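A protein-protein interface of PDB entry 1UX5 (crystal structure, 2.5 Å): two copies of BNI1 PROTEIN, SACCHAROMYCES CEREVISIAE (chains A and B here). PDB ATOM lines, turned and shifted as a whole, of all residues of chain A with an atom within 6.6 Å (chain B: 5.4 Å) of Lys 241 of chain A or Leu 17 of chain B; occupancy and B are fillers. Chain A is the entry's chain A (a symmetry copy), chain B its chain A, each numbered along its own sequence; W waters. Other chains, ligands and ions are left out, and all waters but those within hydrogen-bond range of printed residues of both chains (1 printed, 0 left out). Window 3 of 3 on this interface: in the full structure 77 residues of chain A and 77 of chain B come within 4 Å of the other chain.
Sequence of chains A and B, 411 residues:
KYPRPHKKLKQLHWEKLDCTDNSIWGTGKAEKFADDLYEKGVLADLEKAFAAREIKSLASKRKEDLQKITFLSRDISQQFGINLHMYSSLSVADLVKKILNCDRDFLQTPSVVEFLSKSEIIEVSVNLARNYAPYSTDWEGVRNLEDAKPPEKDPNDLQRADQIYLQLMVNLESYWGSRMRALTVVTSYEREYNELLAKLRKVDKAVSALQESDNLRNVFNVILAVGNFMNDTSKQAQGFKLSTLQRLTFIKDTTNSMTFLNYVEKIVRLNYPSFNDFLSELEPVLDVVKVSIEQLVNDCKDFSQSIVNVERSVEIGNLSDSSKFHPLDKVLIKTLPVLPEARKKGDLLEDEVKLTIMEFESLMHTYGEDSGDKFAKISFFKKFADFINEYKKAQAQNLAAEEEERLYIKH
O of Glu 15 of chain B is in hydrogen-bond range of N of Lys 241 of chain A, at 2.8 Å. OE1 of Glu 15 of chain B lies within hydrogen-bond range of OG of Ser 243 of chain A (3.1 Å). The backbone carbonyl oxygen (O) of Gly 239 of chain A is in hydrogen-bond range of the backbone NH (N) of Leu 17 of chain B (2.9 Å).
The backbone carbonyl oxygen (O) of Lys 241 of chain A lies within hydrogen-bond range of the side-chain hydroxyl (OG1) of Thr 244 of chain A, 2.8 Å away. NZ of Lys 241 of chain A sits at hydrogen-bond distance from O of Gly 368 of chain A (3.3 Å).
Among the printed residues, merely in contact across the chains: Lys 241 of chain A with Leu 17 of chain B (3.1 Å), Gly 239 of chain A with Lys 16 of chain B (3.2 Å), Ala 237 of chain A with Lys 16 of chain B (3.3 Å), Phe 240 of chain A with Glu 15 of chain B (3.4 Å), Phe 240 of chain A with Leu 17 of chain B (3.5 Å), Gly 239 of chain A with Trp 25 of chain B (3.5 Å), Gln 238 of chain A with Trp 25 of chain B (3.5 Å), Phe 240 of chain A with Trp 25 of chain B (3.5 Å), Phe 220 of chain A with Trp 25 of chain B (3.6 Å) and Thr 244 of chain A with Glu 15 of chain B (3.7 Å).
Printed residues of chain B within 4 Å of Ser 243 of chain A: Glu 15 (3.1 Å). Glu 369 of chain A touches none of the printed residues of chain B. Leu 17 of chain B touches just these residues of chain A: Gly 239, Phe 240 and Lys 241. Of the printed residues of chain A, Trp 25 of chain B touches Phe 220, Gln 238, Gly 239 and Phe 240. The nearest residue of chain B that does not touch Lys 241 of chain A is Lys 16 of chain B (4.5 Å). The nearest printed residue of chain B that does not touch Gly 239 of chain A is Glu 15 of chain B (4.5 Å).
Hydrophobic or aromatic side chains of chain B that line the printed part of chain A: Leu 17 and Trp 25. Among the printed residues, no Asp or Glu carboxylate lies within 4 Å of a Lys or Arg side-chain nitrogen of the other chain.
No position is printed for both chains.
Water W1 lies within hydrogen-bond range of the backbone carbonyl oxygen of Leu 17 of chain B, the backbone NH of Gln 238 of chain A and the backbone carbonyl oxygen of Asp 18 of chain B.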
ATOM      1  N   PHE A 220     -22.575  -5.434  20.286  1.00  0.00           N
ATOM      2  CA  PHE A 220     -22.959  -6.418  21.283  1.00  0.00           C
ATOM      3  C   PHE A 220     -23.626  -5.796  22.503  1.00  0.00           C
ATOM      4  O   PHE A 220     -24.519  -6.398  23.102  1.00  0.00           O
ATOM      5  CB  PHE A 220     -21.739  -7.210  21.734  1.00  0.00           C
ATOM      6  CG  PHE A 220     -21.407  -8.376  20.853  1.00  0.00           C
ATOM      7  CD1 PHE A 220     -21.509  -8.279  19.469  1.00  0.00           C
ATOM      8  CD2 PHE A 220     -20.946  -9.567  21.411  1.00  0.00           C
ATOM      9  CE1 PHE A 220     -21.154  -9.356  18.651  1.00  0.00           C
ATOM     10  CE2 PHE A 220     -20.588 -10.651  20.607  1.00  0.00           C
ATOM     11  CZ  PHE A 220     -20.691 -10.546  19.223  1.00  0.00           C
ATOM     12  N   ALA A 237     -29.544 -10.413  31.826  1.00  0.00           N
ATOM     13  CA  ALA A 237     -28.176 -10.899  31.730  1.00  0.00           C
ATOM     14  C   ALA A 237     -27.104  -9.821  31.718  1.00  0.00           C
ATOM     15  O   ALA A 237     -27.326  -8.700  31.246  1.00  0.00           O
ATOM     16  CB  ALA A 237     -28.028 -11.772  30.498  1.00  0.00           C
ATOM     17  N   GLN A 238     -25.935 -10.198  32.237  1.00  0.00           N
ATOM     18  CA  GLN A 238     -24.762  -9.336  32.316  1.00  0.00           C
ATOM     19  C   GLN A 238     -23.970  -9.457  31.017  1.00  0.00           C
ATOM     20  O   GLN A 238     -23.150  -8.599  30.689  1.00  0.00           O
ATOM     21  CB  GLN A 238     -23.882  -9.752  33.498  1.00  0.00           C
ATOM     22  CG  GLN A 238     -24.400  -9.331  34.873  1.00  0.00           C
ATOM     23  CD  GLN A 238     -24.556  -7.818  35.011  1.00  0.00           C
ATOM     24  OE1 GLN A 238     -23.701  -7.050  34.567  1.00  0.00           O
ATOM     25  NE2 GLN A 238     -25.646  -7.389  35.638  1.00  0.00           N
ATOM     26  N   GLY A 239     -24.227 -10.535  30.284  1.00  0.00           N
ATOM     27  CA  GLY A 239     -23.560 -10.763  29.013  1.00  0.00           C
ATOM     28  C   GLY A 239     -24.170 -11.991  28.372  1.00  0.00           C
ATOM     29  O   GLY A 239     -24.956 -12.693  29.011  1.00  0.00           O
ATOM     30  N   PHE A 240     -23.837 -12.268  27.118  1.00  0.00           N
ATOM     31  CA  PHE A 240     -24.402 -13.450  26.495  1.00  0.00           C
ATOM     32  C   PHE A 240     -23.395 -14.214  25.654  1.00  0.00           C
ATOM     33  O   PHE A 240     -22.390 -13.650  25.213  1.00  0.00           O
ATOM     34  CB  PHE A 240     -25.635 -13.069  25.664  1.00  0.00           C
ATOM     35  CG  PHE A 240     -25.367 -12.067  24.575  1.00  0.00           C
ATOM     36  CD1 PHE A 240     -24.634 -12.416  23.441  1.00  0.00           C
ATOM     37  CD2 PHE A 240     -25.870 -10.778  24.671  1.00  0.00           C
ATOM     38  CE1 PHE A 240     -24.408 -11.487  22.415  1.00  0.00           C
ATOM     39  CE2 PHE A 240     -25.653  -9.833  23.649  1.00  0.00           C
ATOM     40  CZ  PHE A 240     -24.923 -10.189  22.524  1.00  0.00           C
ATOM     41  N   LYS A 241     -23.652 -15.506  25.449  1.00  0.00           N
ATOM     42  CA  LYS A 241     -22.762 -16.334  24.644  1.00  0.00           C
ATOM     43  C   LYS A 241     -23.011 -16.079  23.157  1.00  0.00           C
ATOM     44  O   LYS A 241     -24.031 -15.493  22.771  1.00  0.00           O
ATOM     45  CB  LYS A 241     -22.978 -17.810  24.955  1.00  0.00           C
ATOM     46  CG  LYS A 241     -22.886 -18.144  26.422  1.00  0.00           C
ATOM     47  CD  LYS A 241     -22.918 -19.649  26.630  1.00  0.00           C
ATOM     48  CE  LYS A 241     -21.521 -20.214  26.652  1.00  0.00           C
ATOM     49  NZ  LYS A 241     -20.798 -19.647  27.816  1.00  0.00           N
ATOM     50  N   LEU A 242     -22.075 -16.523  22.324  1.00  0.00           N
ATOM     51  CA  LEU A 242     -22.182 -16.321  20.886  1.00  0.00           C
ATOM     52  C   LEU A 242     -23.386 -17.004  20.269  1.00  0.00           C
ATOM     53  O   LEU A 242     -23.890 -16.554  19.236  1.00  0.00           O
ATOM     54  CB  LEU A 242     -20.918 -16.807  20.195  1.00  0.00           C
ATOM     55  CG  LEU A 242     -19.631 -16.077  20.560  1.00  0.00           C
ATOM     56  CD1 LEU A 242     -18.528 -16.604  19.660  1.00  0.00           C
ATOM     57  CD2 LEU A 242     -19.792 -14.571  20.386  1.00  0.00           C
ATOM     58  N   SER A 243     -23.844 -18.092  20.882  1.00  0.00           N
ATOM     59  CA  SER A 243     -25.007 -18.802  20.360  1.00  0.00           C
ATOM     60  C   SER A 243     -26.122 -17.787  20.159  1.00  0.00           C
ATOM     61  O   SER A 243     -26.945 -17.910  19.256  1.00  0.00           O
ATOM     62  CB  SER A 243     -25.464 -19.872  21.346  1.00  0.00           C
ATOM     63  OG  SER A 243     -25.659 -19.312  22.628  1.00  0.00           O
ATOM     64  N   THR A 244     -26.125 -16.770  21.005  1.00  0.00           N
ATOM     65  CA  THR A 244     -27.123 -15.716  20.946  1.00  0.00           C
ATOM     66  C   THR A 244     -27.246 -15.060  19.570  1.00  0.00           C
ATOM     67  O   THR A 244     -28.344 -14.710  19.125  1.00  0.00           O
ATOM     68  CB  THR A 244     -26.792 -14.615  21.969  1.00  0.00           C
ATOM     69  OG1 THR A 244     -26.786 -15.184  23.286  1.00  0.00           O
ATOM     70  CG2 THR A 244     -27.817 -13.472  21.884  1.00  0.00           C
ATOM     71  N   LEU A 245     -26.112 -14.883  18.908  1.00  0.00           N
ATOM     72  CA  LEU A 245     -26.084 -14.243  17.603  1.00  0.00           C
ATOM     73  C   LEU A 245     -26.959 -14.942  16.572  1.00  0.00           C
ATOM     74  O   LEU A 245     -27.695 -14.296  15.823  1.00  0.00           O
ATOM     75  CB  LEU A 245     -24.648 -14.181  17.083  1.00  0.00           C
ATOM     76  CG  LEU A 245     -23.626 -13.371  17.882  1.00  0.00           C
ATOM     77  CD1 LEU A 245     -22.400 -13.129  17.002  1.00  0.00           C
ATOM     78  CD2 LEU A 245     -24.230 -12.031  18.305  1.00  0.00           C
ATOM     79  N   THR A 366     -12.202 -14.421  25.831  1.00  0.00           N
ATOM     80  CA  THR A 366     -12.725 -13.068  25.828  1.00  0.00           C
ATOM     81  C   THR A 366     -14.217 -13.036  25.501  1.00  0.00           C
ATOM     82  O   THR A 366     -14.947 -12.179  26.008  1.00  0.00           O
ATOM     83  CB  THR A 366     -11.967 -12.215  24.816  1.00  0.00           C
ATOM     84  OG1 THR A 366     -10.789 -11.704  25.440  1.00  0.00           O
ATOM     85  CG2 THR A 366     -12.820 -11.077  24.306  1.00  0.00           C
ATOM     86  N   TYR A 367     -14.662 -13.961  24.652  1.00  0.00           N
ATOM     87  CA  TYR A 367     -16.069 -14.016  24.279  1.00  0.00           C
ATOM     88  C   TYR A 367     -16.807 -15.142  24.984  1.00  0.00           C
ATOM     89  O   TYR A 367     -17.881 -15.556  24.550  1.00  0.00           O
ATOM     90  CB  TYR A 367     -16.231 -14.149  22.753  1.00  0.00           C
ATOM     91  CG  TYR A 367     -15.899 -12.873  22.006  1.00  0.00           C
ATOM     92  CD1 TYR A 367     -14.586 -12.566  21.673  1.00  0.00           C
ATOM     93  CD2 TYR A 367     -16.891 -11.942  21.687  1.00  0.00           C
ATOM     94  CE1 TYR A 367     -14.260 -11.363  21.045  1.00  0.00           C
ATOM     95  CE2 TYR A 367     -16.575 -10.728  21.055  1.00  0.00           C
ATOM     96  CZ  TYR A 367     -15.252 -10.445  20.740  1.00  0.00           C
ATOM     97  OH  TYR A 367     -14.899  -9.242  20.153  1.00  0.00           O
ATOM     98  N   GLY A 368     -16.222 -15.639  26.067  1.00  0.00           N
ATOM     99  CA  GLY A 368     -16.855 -16.701  26.836  1.00  0.00           C
ATOM    100  C   GLY A 368     -16.944 -18.108  26.253  1.00  0.00           C
ATOM    101  O   GLY A 368     -17.817 -18.883  26.646  1.00  0.00           O
ATOM    102  N   GLU A 369     -16.060 -18.460  25.328  1.00  0.00           N
ATOM    103  CA  GLU A 369     -16.089 -19.801  24.745  1.00  0.00           C
ATOM    104  C   GLU A 369     -14.997 -20.658  25.381  1.00  0.00           C
ATOM    105  O   GLU A 369     -13.973 -20.136  25.818  1.00  0.00           O
ATOM    106  CB  GLU A 369     -15.883 -19.721  23.232  1.00  0.00           C
ATOM    107  CG  GLU A 369     -16.933 -18.892  22.514  1.00  0.00           C
ATOM    108  CD  GLU A 369     -18.325 -19.503  22.603  1.00  0.00           C
ATOM    109  OE1 GLU A 369     -18.515 -20.637  22.100  1.00  0.00           O
ATOM    110  OE2 GLU A 369     -19.227 -18.847  23.177  1.00  0.00           O
ATOM    111  N   ASP A 370     -15.210 -21.967  25.441  1.00  0.00           N
ATOM    112  CA  ASP A 370     -14.212 -22.844  26.040  1.00  0.00           C
ATOM    113  C   ASP A 370     -13.137 -23.277  25.040  1.00  0.00           C
ATOM    114  O   ASP A 370     -13.431 -23.938  24.042  1.00  0.00           O
ATOM    115  CB  ASP A 370     -14.882 -24.079  26.646  1.00  0.00           C
ATOM    116  CG  ASP A 370     -13.879 -25.065  27.202  1.00  0.00           C
ATOM    117  OD1 ASP A 370     -13.011 -24.647  27.999  1.00  0.00           O
ATOM    118  OD2 ASP A 370     -13.960 -26.258  26.842  1.00  0.00           O
ATOM    119  N   GLU B  15     -28.343 -17.368  25.861  1.00  0.00           N
ATOM    120  CA  GLU B  15     -27.631 -18.102  26.903  1.00  0.00           C
ATOM    121  C   GLU B  15     -26.751 -17.025  27.515  1.00  0.00           C
ATOM    122  O   GLU B  15     -25.857 -16.492  26.854  1.00  0.00           O
ATOM    123  CB  GLU B  15     -26.755 -19.209  26.325  1.00  0.00           C
ATOM    124  CG  GLU B  15     -27.478 -20.198  25.450  1.00  0.00           C
ATOM    125  CD  GLU B  15     -26.644 -21.438  25.203  1.00  0.00           C
ATOM    126  OE1 GLU B  15     -25.422 -21.292  24.961  1.00  0.00           O
ATOM    127  OE2 GLU B  15     -27.210 -22.554  25.249  1.00  0.00           O
ATOM    128  N   LYS B  16     -27.009 -16.676  28.764  1.00  0.00           N
ATOM    129  CA  LYS B  16     -26.227 -15.623  29.384  1.00  0.00           C
ATOM    130  C   LYS B  16     -24.899 -16.082  29.941  1.00  0.00           C
ATOM    131  O   LYS B  16     -24.787 -17.191  30.470  1.00  0.00           O
ATOM    132  CB  LYS B  16     -27.038 -14.947  30.491  1.00  0.00           C
ATOM    133  CG  LYS B  16     -28.188 -15.775  31.034  1.00  0.00           C
ATOM    134  CD  LYS B  16     -28.849 -15.051  32.194  1.00  0.00           C
ATOM    135  CE  LYS B  16     -30.045 -15.815  32.745  1.00  0.00           C
ATOM    136  NZ  LYS B  16     -30.549 -15.169  33.995  1.00  0.00           N
ATOM    137  N   LEU B  17     -23.880 -15.241  29.767  1.00  0.00           N
ATOM    138  CA  LEU B  17     -22.571 -15.528  30.324  1.00  0.00           C
ATOM    139  C   LEU B  17     -22.897 -15.079  31.719  1.00  0.00           C
ATOM    140  O   LEU B  17     -23.383 -13.965  31.915  1.00  0.00           O
ATOM    141  CB  LEU B  17     -21.483 -14.657  29.707  1.00  0.00           C
ATOM    142  CG  LEU B  17     -21.132 -15.090  28.287  1.00  0.00           C
ATOM    143  CD1 LEU B  17     -20.012 -14.223  27.739  1.00  0.00           C
ATOM    144  CD2 LEU B  17     -20.725 -16.555  28.293  1.00  0.00           C
ATOM    145  N   ASP B  18     -22.666 -15.971  32.674  1.00  0.00           N
ATOM    146  CA  ASP B  18     -22.996 -15.747  34.075  1.00  0.00           C
ATOM    147  C   ASP B  18     -22.450 -14.506  34.759  1.00  0.00           C
ATOM    148  O   ASP B  18     -23.188 -13.824  35.473  1.00  0.00           O
ATOM    149  CB  ASP B  18     -22.631 -17.000  34.874  1.00  0.00           C
ATOM    150  CG  ASP B  18     -23.309 -18.251  34.327  1.00  0.00           C
ATOM    151  OD1 ASP B  18     -24.559 -18.299  34.315  1.00  0.00           O
ATOM    152  OD2 ASP B  18     -22.592 -19.181  33.899  1.00  0.00           O
ATOM    153  N   CYS B  19     -21.178 -14.193  34.549  1.00  0.00           N
ATOM    154  CA  CYS B  19     -20.635 -13.017  35.209  1.00  0.00           C
ATOM    155  C   CYS B  19     -19.657 -12.182  34.392  1.00  0.00           C
ATOM    156  O   CYS B  19     -18.931 -12.688  33.536  1.00  0.00           O
ATOM    157  CB  CYS B  19     -19.977 -13.431  36.531  1.00  0.00           C
ATOM    158  SG  CYS B  19     -19.506 -12.050  37.617  1.00  0.00           S
ATOM    159  N   TRP B  25     -17.647  -8.024  28.579  1.00  0.00           N
ATOM    160  CA  TRP B  25     -18.836  -7.544  29.280  1.00  0.00           C
ATOM    161  C   TRP B  25     -18.523  -6.835  30.583  1.00  0.00           C
ATOM    162  O   TRP B  25     -17.449  -7.014  31.161  1.00  0.00           O
ATOM    163  CB  TRP B  25     -19.801  -8.704  29.565  1.00  0.00           C
ATOM    164  CG  TRP B  25     -20.197  -9.465  28.337  1.00  0.00           C
ATOM    165  CD1 TRP B  25     -19.751 -10.696  27.960  1.00  0.00           C
ATOM    166  CD2 TRP B  25     -21.050  -9.006  27.280  1.00  0.00           C
ATOM    167  NE1 TRP B  25     -20.270 -11.034  26.730  1.00  0.00           N
ATOM    168  CE2 TRP B  25     -21.070 -10.016  26.290  1.00  0.00           C
ATOM    169  CE3 TRP B  25     -21.795  -7.839  27.075  1.00  0.00           C
ATOM    170  CZ2 TRP B  25     -21.807  -9.899  25.110  1.00  0.00           C
ATOM    171  CZ3 TRP B  25     -22.533  -7.716  25.893  1.00  0.00           C
ATOM    172  CH2 TRP B  25     -22.533  -8.744  24.926  1.00  0.00           C
HETATM  173  O   HOH W   1     -25.438 -13.036  33.249  1.00  0.00           O
